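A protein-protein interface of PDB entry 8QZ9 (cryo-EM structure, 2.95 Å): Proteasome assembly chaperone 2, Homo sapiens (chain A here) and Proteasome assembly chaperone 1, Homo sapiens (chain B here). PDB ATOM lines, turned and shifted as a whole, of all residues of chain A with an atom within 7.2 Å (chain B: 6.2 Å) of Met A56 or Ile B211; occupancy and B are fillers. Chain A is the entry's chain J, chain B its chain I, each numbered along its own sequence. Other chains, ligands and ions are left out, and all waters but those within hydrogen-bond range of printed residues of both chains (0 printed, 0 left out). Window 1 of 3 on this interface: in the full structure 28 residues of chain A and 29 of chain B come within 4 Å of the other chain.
The backbone carbonyl oxygen (O) of Val B212 lies within hydrogen-bond range of the backbone NH (N) of Val A57, at 3.0 Å.
Of chain B, only Ile B211, Val B212, Ala B217 and Ser B221 come within 4 Å of Met A56.
Asn B210 touches none of the printed residues of chain A.
Ile B211 touches just these residues of chain A: Met A56 (3.7 Å) and Val A57 (3.4 Å).
Of the printed residues of chain A, Asp B214 touches Pro A55.
Of the printed residues of chain A, Ser B221 touches Met A56 and Val A57.
Tyr B236 touches none of the printed residues of chain A.
The nearest residue of chain B that does not touch Met A56 is His B213 (4.3 Å).
The nearest residue of chain A that does not touch Ile B211 is Gly A58 (4.8 Å).
Hydrophobic or aromatic side chains of chain A that line the printed part of chain B: Pro A55, Met A56 and Val A57.
Along chain A the printed residues that touch a printed residue of chain B span positions 55 to 59.
Among the printed residues, no Asp or Glu carboxylate lies within 4 Å of a Lys or Arg side-chain nitrogen of the other chain.
OG of Ser B221 lies within hydrogen-bond range of O of Ala B217 (2.5 Å).
Among the printed residues, pairs that only touch across the chains: Met A56 with Val B212, Val A57 with Ser B221, Val A57 with Ile B211, Pro A55 with His B213, Met A56 with Ile B211, Asn A59 with Gln B208, Val A57 with Ala B217, Pro A55 with Ala B218, Met A56 with Ala B217, Met A56 with Ser B221 and Pro A55 with Asp B214.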
ATOM      1  N   LEU A  53     -19.332  30.805   9.350  1.00  0.00           N
ATOM      2  CA  LEU A  53     -19.330  31.596  10.571  1.00  0.00           C
ATOM      3  C   LEU A  53     -18.730  30.784  11.709  1.00  0.00           C
ATOM      4  O   LEU A  53     -18.903  29.563  11.770  1.00  0.00           O
ATOM      5  CB  LEU A  53     -20.747  32.042  10.940  1.00  0.00           C
ATOM      6  CG  LEU A  53     -21.263  33.315  10.269  1.00  0.00           C
ATOM      7  CD1 LEU A  53     -22.774  33.273  10.146  1.00  0.00           C
ATOM      8  CD2 LEU A  53     -20.823  34.543  11.043  1.00  0.00           C
ATOM      9  N   VAL A  54     -18.025  31.467  12.604  1.00  0.00           N
ATOM     10  CA  VAL A  54     -17.388  30.783  13.736  1.00  0.00           C
ATOM     11  C   VAL A  54     -18.466  30.185  14.630  1.00  0.00           C
ATOM     12  O   VAL A  54     -19.409  30.899  15.026  1.00  0.00           O
ATOM     13  CB  VAL A  54     -16.500  31.759  14.523  1.00  0.00           C
ATOM     14  CG1 VAL A  54     -15.932  31.082  15.756  1.00  0.00           C
ATOM     15  CG2 VAL A  54     -15.385  32.287  13.639  1.00  0.00           C
ATOM     16  N   PRO A  55     -18.393  28.901  14.973  1.00  0.00           N
ATOM     17  CA  PRO A  55     -19.451  28.294  15.785  1.00  0.00           C
ATOM     18  C   PRO A  55     -19.475  28.836  17.204  1.00  0.00           C
ATOM     19  O   PRO A  55     -18.448  29.216  17.772  1.00  0.00           O
ATOM     20  CB  PRO A  55     -19.096  26.803  15.768  1.00  0.00           C
ATOM     21  CG  PRO A  55     -17.638  26.768  15.498  1.00  0.00           C
ATOM     22  CD  PRO A  55     -17.356  27.927  14.596  1.00  0.00           C
ATOM     23  N   MET A  56     -20.676  28.869  17.775  1.00  0.00           N
ATOM     24  CA  MET A  56     -20.875  29.272  19.160  1.00  0.00           C
ATOM     25  C   MET A  56     -22.208  28.712  19.632  1.00  0.00           C
ATOM     26  O   MET A  56     -23.100  28.433  18.828  1.00  0.00           O
ATOM     27  CB  MET A  56     -20.813  30.797  19.316  1.00  0.00           C
ATOM     28  CG  MET A  56     -21.865  31.581  18.539  1.00  0.00           C
ATOM     29  SD  MET A  56     -23.509  31.645  19.273  1.00  0.00           S
ATOM     30  CE  MET A  56     -23.205  32.713  20.674  1.00  0.00           C
ATOM     31  N   VAL A  57     -22.332  28.542  20.950  1.00  0.00           N
ATOM     32  CA  VAL A  57     -23.537  27.985  21.550  1.00  0.00           C
ATOM     33  C   VAL A  57     -23.863  28.733  22.835  1.00  0.00           C
ATOM     34  O   VAL A  57     -23.000  29.335  23.474  1.00  0.00           O
ATOM     35  CB  VAL A  57     -23.405  26.474  21.842  1.00  0.00           C
ATOM     36  CG1 VAL A  57     -23.498  25.677  20.557  1.00  0.00           C
ATOM     37  CG2 VAL A  57     -22.103  26.186  22.560  1.00  0.00           C
ATOM     38  N   GLY A  58     -25.134  28.677  23.210  1.00  0.00           N
ATOM     39  CA  GLY A  58     -25.599  29.309  24.429  1.00  0.00           C
ATOM     40  C   GLY A  58     -27.059  28.978  24.642  1.00  0.00           C
ATOM     41  O   GLY A  58     -27.725  28.408  23.773  1.00  0.00           O
ATOM     42  N   ASN A  59     -27.553  29.351  25.817  1.00  0.00           N
ATOM     43  CA  ASN A  59     -28.941  29.088  26.171  1.00  0.00           C
ATOM     44  C   ASN A  59     -29.841  30.105  25.471  1.00  0.00           C
ATOM     45  O   ASN A  59     -29.401  30.877  24.617  1.00  0.00           O
ATOM     46  CB  ASN A  59     -29.112  29.099  27.686  1.00  0.00           C
ATOM     47  CG  ASN A  59     -29.114  27.704  28.280  1.00  0.00           C
ATOM     48  OD1 ASN A  59     -29.242  26.711  27.565  1.00  0.00           O
ATOM     49  ND2 ASN A  59     -28.973  27.623  29.597  1.00  0.00           N
ATOM     50  N   LEU A  72     -31.332  25.647  23.740  1.00  0.00           N
ATOM     51  CA  LEU A  72     -30.032  25.912  23.144  1.00  0.00           C
ATOM     52  C   LEU A  72     -30.184  26.689  21.841  1.00  0.00           C
ATOM     53  O   LEU A  72     -31.156  26.521  21.100  1.00  0.00           O
ATOM     54  CB  LEU A  72     -29.286  24.604  22.893  1.00  0.00           C
ATOM     55  CG  LEU A  72     -27.778  24.707  22.657  1.00  0.00           C
ATOM     56  CD1 LEU A  72     -27.076  25.214  23.900  1.00  0.00           C
ATOM     57  CD2 LEU A  72     -27.213  23.366  22.234  1.00  0.00           C
ATOM     58  N   SER A  73     -29.206  27.550  21.565  1.00  0.00           N
ATOM     59  CA  SER A  73     -29.216  28.376  20.369  1.00  0.00           C
ATOM     60  C   SER A  73     -27.843  28.340  19.714  1.00  0.00           C
ATOM     61  O   SER A  73     -26.829  28.115  20.377  1.00  0.00           O
ATOM     62  CB  SER A  73     -29.608  29.825  20.685  1.00  0.00           C
ATOM     63  OG  SER A  73     -30.984  29.918  21.008  1.00  0.00           O
ATOM     64  N   ILE A  74     -27.822  28.569  18.402  1.00  0.00           N
ATOM     65  CA  ILE A  74     -26.585  28.551  17.631  1.00  0.00           C
ATOM     66  C   ILE A  74     -26.392  29.906  16.961  1.00  0.00           C
ATOM     67  O   ILE A  74     -27.195  30.825  17.156  1.00  0.00           O
ATOM     68  CB  ILE A  74     -26.582  27.408  16.598  1.00  0.00           C
ATOM     69  CG1 ILE A  74     -27.537  27.717  15.449  1.00  0.00           C
ATOM     70  CG2 ILE A  74     -26.965  26.096  17.257  1.00  0.00           C
ATOM     71  CD1 ILE A  74     -27.385  26.782  14.273  1.00  0.00           C
ATOM     72  N   ASN A  75     -25.322  30.040  16.175  1.00  0.00           N
ATOM     73  CA  ASN A  75     -24.950  31.347  15.640  1.00  0.00           C
ATOM     74  C   ASN A  75     -25.984  31.887  14.656  1.00  0.00           C
ATOM     75  O   ASN A  75     -26.242  33.095  14.627  1.00  0.00           O
ATOM     76  CB  ASN A  75     -23.563  31.272  14.997  1.00  0.00           C
ATOM     77  CG  ASN A  75     -23.492  30.278  13.855  1.00  0.00           C
ATOM     78  OD1 ASN A  75     -24.501  29.710  13.443  1.00  0.00           O
ATOM     79  ND2 ASN A  75     -22.289  30.060  13.341  1.00  0.00           N
ATOM     80  N   ALA A  76     -26.582  31.023  13.840  1.00  0.00           N
ATOM     81  CA  ALA A  76     -27.550  31.441  12.834  1.00  0.00           C
ATOM     82  C   ALA A  76     -28.899  30.797  13.115  1.00  0.00           C
ATOM     83  O   ALA A  76     -28.988  29.576  13.266  1.00  0.00           O
ATOM     84  CB  ALA A  76     -27.073  31.074  11.428  1.00  0.00           C
ATOM     85  N   ARG A  92     -24.913  35.725  15.150  1.00  0.00           N
ATOM     86  CA  ARG A  92     -24.290  36.053  16.428  1.00  0.00           C
ATOM     87  C   ARG A  92     -22.791  35.782  16.435  1.00  0.00           C
ATOM     88  O   ARG A  92     -22.208  35.608  17.509  1.00  0.00           O
ATOM     89  CB  ARG A  92     -24.954  35.276  17.567  1.00  0.00           C
ATOM     90  CG  ARG A  92     -26.441  35.514  17.705  1.00  0.00           C
ATOM     91  CD  ARG A  92     -26.996  34.771  18.904  1.00  0.00           C
ATOM     92  NE  ARG A  92     -28.389  35.116  19.159  1.00  0.00           N
ATOM     93  CZ  ARG A  92     -29.426  34.456  18.664  1.00  0.00           C
ATOM     94  NH1 ARG A  92     -29.265  33.404  17.880  1.00  0.00           N
ATOM     95  NH2 ARG A  92     -30.656  34.862  18.963  1.00  0.00           N
ATOM     96  N   SER A  93     -22.148  35.745  15.272  1.00  0.00           N
ATOM     97  CA  SER A  93     -20.734  35.408  15.197  1.00  0.00           C
ATOM     98  C   SER A  93     -20.068  36.306  14.164  1.00  0.00           C
ATOM     99  O   SER A  93     -20.636  37.306  13.717  1.00  0.00           O
ATOM    100  CB  SER A  93     -20.544  33.923  14.868  1.00  0.00           C
ATOM    101  OG  SER A  93     -20.650  33.130  16.033  1.00  0.00           O
ATOM    102  N   ILE A  94     -18.846  35.939  13.789  1.00  0.00           N
ATOM    103  CA  ILE A  94     -18.019  36.717  12.877  1.00  0.00           C
ATOM    104  C   ILE A  94     -17.550  35.814  11.745  1.00  0.00           C
ATOM    105  O   ILE A  94     -17.264  34.630  11.958  1.00  0.00           O
ATOM    106  CB  ILE A  94     -16.825  37.354  13.618  1.00  0.00           C
ATOM    107  CG1 ILE A  94     -15.954  36.270  14.249  1.00  0.00           C
ATOM    108  CG2 ILE A  94     -17.311  38.330  14.673  1.00  0.00           C
ATOM    109  CD1 ILE A  94     -14.668  36.781  14.816  1.00  0.00           C
ATOM    110  N   GLU B 207     -25.338  29.937  32.784  1.00  0.00           N
ATOM    111  CA  GLU B 207     -26.218  31.083  32.945  1.00  0.00           C
ATOM    112  C   GLU B 207     -26.472  31.753  31.596  1.00  0.00           C
ATOM    113  O   GLU B 207     -26.019  31.295  30.544  1.00  0.00           O
ATOM    114  CB  GLU B 207     -25.626  32.063  33.952  1.00  0.00           C
ATOM    115  CG  GLU B 207     -25.992  31.753  35.393  1.00  0.00           C
ATOM    116  CD  GLU B 207     -25.414  30.436  35.871  1.00  0.00           C
ATOM    117  OE1 GLU B 207     -24.269  30.115  35.493  1.00  0.00           O
ATOM    118  OE2 GLU B 207     -26.105  29.721  36.626  1.00  0.00           O
ATOM    119  N   GLN B 208     -27.210  32.860  31.630  1.00  0.00           N
ATOM    120  CA  GLN B 208     -27.731  33.442  30.399  1.00  0.00           C
ATOM    121  C   GLN B 208     -26.665  34.165  29.578  1.00  0.00           C
ATOM    122  O   GLN B 208     -26.462  33.806  28.412  1.00  0.00           O
ATOM    123  CB  GLN B 208     -28.900  34.381  30.702  1.00  0.00           C
ATOM    124  CG  GLN B 208     -30.235  33.669  30.863  1.00  0.00           C
ATOM    125  CD  GLN B 208     -30.335  32.408  30.028  1.00  0.00           C
ATOM    126  OE1 GLN B 208     -30.257  32.452  28.803  1.00  0.00           O
ATOM    127  NE2 GLN B 208     -30.511  31.274  30.691  1.00  0.00           N
ATOM    128  N   PRO B 209     -25.959  35.183  30.113  1.00  0.00           N
ATOM    129  CA  PRO B 209     -25.021  35.915  29.253  1.00  0.00           C
ATOM    130  C   PRO B 209     -23.658  35.249  29.154  1.00  0.00           C
ATOM    131  O   PRO B 209     -22.629  35.923  29.250  1.00  0.00           O
ATOM    132  CB  PRO B 209     -24.924  37.280  29.939  1.00  0.00           C
ATOM    133  CG  PRO B 209     -25.087  36.962  31.382  1.00  0.00           C
ATOM    134  CD  PRO B 209     -25.914  35.694  31.495  1.00  0.00           C
ATOM    135  N   ASN B 210     -23.633  33.934  28.946  1.00  0.00           N
ATOM    136  CA  ASN B 210     -22.394  33.182  28.811  1.00  0.00           C
ATOM    137  C   ASN B 210     -22.479  32.314  27.568  1.00  0.00           C
ATOM    138  O   ASN B 210     -23.503  31.667  27.330  1.00  0.00           O
ATOM    139  CB  ASN B 210     -22.128  32.315  30.045  1.00  0.00           C
ATOM    140  CG  ASN B 210     -21.704  33.128  31.249  1.00  0.00           C
ATOM    141  OD1 ASN B 210     -20.604  33.675  31.287  1.00  0.00           O
ATOM    142  ND2 ASN B 210     -22.575  33.206  32.244  1.00  0.00           N
ATOM    143  N   ILE B 211     -21.403  32.296  26.778  1.00  0.00           N
ATOM    144  CA  ILE B 211     -21.359  31.538  25.537  1.00  0.00           C
ATOM    145  C   ILE B 211     -20.064  30.742  25.479  1.00  0.00           C
ATOM    146  O   ILE B 211     -19.090  31.037  26.175  1.00  0.00           O
ATOM    147  CB  ILE B 211     -21.483  32.443  24.293  1.00  0.00           C
ATOM    148  CG1 ILE B 211     -20.339  33.454  24.253  1.00  0.00           C
ATOM    149  CG2 ILE B 211     -22.816  33.160  24.285  1.00  0.00           C
ATOM    150  CD1 ILE B 211     -20.140  34.085  22.900  1.00  0.00           C
ATOM    151  N   VAL B 212     -20.069  29.714  24.633  1.00  0.00           N
ATOM    152  CA  VAL B 212     -18.915  28.853  24.407  1.00  0.00           C
ATOM    153  C   VAL B 212     -18.659  28.776  22.910  1.00  0.00           C
ATOM    154  O   VAL B 212     -19.601  28.670  22.118  1.00  0.00           O
ATOM    155  CB  VAL B 212     -19.132  27.442  24.992  1.00  0.00           C
ATOM    156  CG1 VAL B 212     -17.855  26.629  24.912  1.00  0.00           C
ATOM    157  CG2 VAL B 212     -19.621  27.528  26.424  1.00  0.00           C
ATOM    158  N   HIS B 213     -17.385  28.837  22.518  1.00  0.00           N
ATOM    159  CA  HIS B 213     -17.031  28.736  21.107  1.00  0.00           C
ATOM    160  C   HIS B 213     -15.982  27.654  20.871  1.00  0.00           C
ATOM    161  O   HIS B 213     -15.711  26.845  21.763  1.00  0.00           O
ATOM    162  CB  HIS B 213     -16.543  30.085  20.575  1.00  0.00           C
ATOM    163  CG  HIS B 213     -15.384  30.654  21.331  1.00  0.00           C
ATOM    164  ND1 HIS B 213     -15.515  31.215  22.582  1.00  0.00           N
ATOM    165  CD2 HIS B 213     -14.074  30.761  21.005  1.00  0.00           C
ATOM    166  CE1 HIS B 213     -14.335  31.636  22.999  1.00  0.00           C
ATOM    167  NE2 HIS B 213     -13.444  31.374  22.060  1.00  0.00           N
ATOM    168  N   ASP B 214     -15.421  27.622  19.659  1.00  0.00           N
ATOM    169  CA  ASP B 214     -14.414  26.654  19.228  1.00  0.00           C
ATOM    170  C   ASP B 214     -14.989  25.252  19.058  1.00  0.00           C
ATOM    171  O   ASP B 214     -16.186  25.093  18.801  1.00  0.00           O
ATOM    172  CB  ASP B 214     -13.222  26.624  20.190  1.00  0.00           C
ATOM    173  CG  ASP B 214     -12.383  27.884  20.117  1.00  0.00           C
ATOM    174  OD1 ASP B 214     -12.336  28.505  19.035  1.00  0.00           O
ATOM    175  OD2 ASP B 214     -11.764  28.249  21.139  1.00  0.00           O
ATOM    176  N   ALA B 217     -18.205  23.800  20.804  1.00  0.00           N
ATOM    177  CA  ALA B 217     -19.368  24.483  20.254  1.00  0.00           C
ATOM    178  C   ALA B 217     -19.735  23.928  18.888  1.00  0.00           C
ATOM    179  O   ALA B 217     -20.919  23.759  18.579  1.00  0.00           O
ATOM    180  CB  ALA B 217     -19.105  25.984  20.167  1.00  0.00           C
ATOM    181  N   ALA B 218     -18.736  23.639  18.053  1.00  0.00           N
ATOM    182  CA  ALA B 218     -19.009  23.073  16.736  1.00  0.00           C
ATOM    183  C   ALA B 218     -19.683  21.712  16.853  1.00  0.00           C
ATOM    184  O   ALA B 218     -20.670  21.430  16.161  1.00  0.00           O
ATOM    185  CB  ALA B 218     -17.713  22.967  15.933  1.00  0.00           C
ATOM    186  N   SER B 221     -23.265  22.163  18.150  1.00  0.00           N
ATOM    187  CA  SER B 221     -24.130  22.724  17.119  1.00  0.00           C
ATOM    188  C   SER B 221     -24.492  21.678  16.075  1.00  0.00           C
ATOM    189  O   SER B 221     -25.645  21.605  15.636  1.00  0.00           O
ATOM    190  CB  SER B 221     -23.451  23.923  16.461  1.00  0.00           C
ATOM    191  OG  SER B 221     -22.901  24.791  17.435  1.00  0.00           O
ATOM    192  N   LEU B 234     -18.456  21.764  31.302  1.00  0.00           N
ATOM    193  CA  LEU B 234     -17.410  22.771  31.404  1.00  0.00           C
ATOM    194  C   LEU B 234     -16.898  22.838  32.833  1.00  0.00           C
ATOM    195  O   LEU B 234     -17.684  22.831  33.784  1.00  0.00           O
ATOM    196  CB  LEU B 234     -17.912  24.153  30.985  1.00  0.00           C
ATOM    197  CG  LEU B 234     -18.093  24.432  29.497  1.00  0.00           C
ATOM    198  CD1 LEU B 234     -19.463  23.976  29.037  1.00  0.00           C
ATOM    199  CD2 LEU B 234     -17.887  25.906  29.210  1.00  0.00           C
ATOM    200  N   TYR B 236     -14.600  25.291  35.231  1.00  0.00           N
ATOM    201  CA  TYR B 236     -13.994  26.606  35.380  1.00  0.00           C
ATOM    202  C   TYR B 236     -12.980  26.546  36.514  1.00  0.00           C
ATOM    203  O   TYR B 236     -13.352  26.326  37.670  1.00  0.00           O
ATOM    204  CB  TYR B 236     -15.055  27.669  35.651  1.00  0.00           C
ATOM    205  CG  TYR B 236     -15.884  28.021  34.438  1.00  0.00           C
ATOM    206  CD1 TYR B 236     -17.028  27.303  34.126  1.00  0.00           C
ATOM    207  CD2 TYR B 236     -15.519  29.065  33.605  1.00  0.00           C
ATOM    208  CE1 TYR B 236     -17.786  27.619  33.019  1.00  0.00           C
ATOM    209  CE2 TYR B 236     -16.271  29.387  32.497  1.00  0.00           C
ATOM    210  CZ  TYR B 236     -17.403  28.661  32.209  1.00  0.00           C
ATOM    211  OH  TYR B 236     -18.154  28.981  31.103  1.00  0.00           O
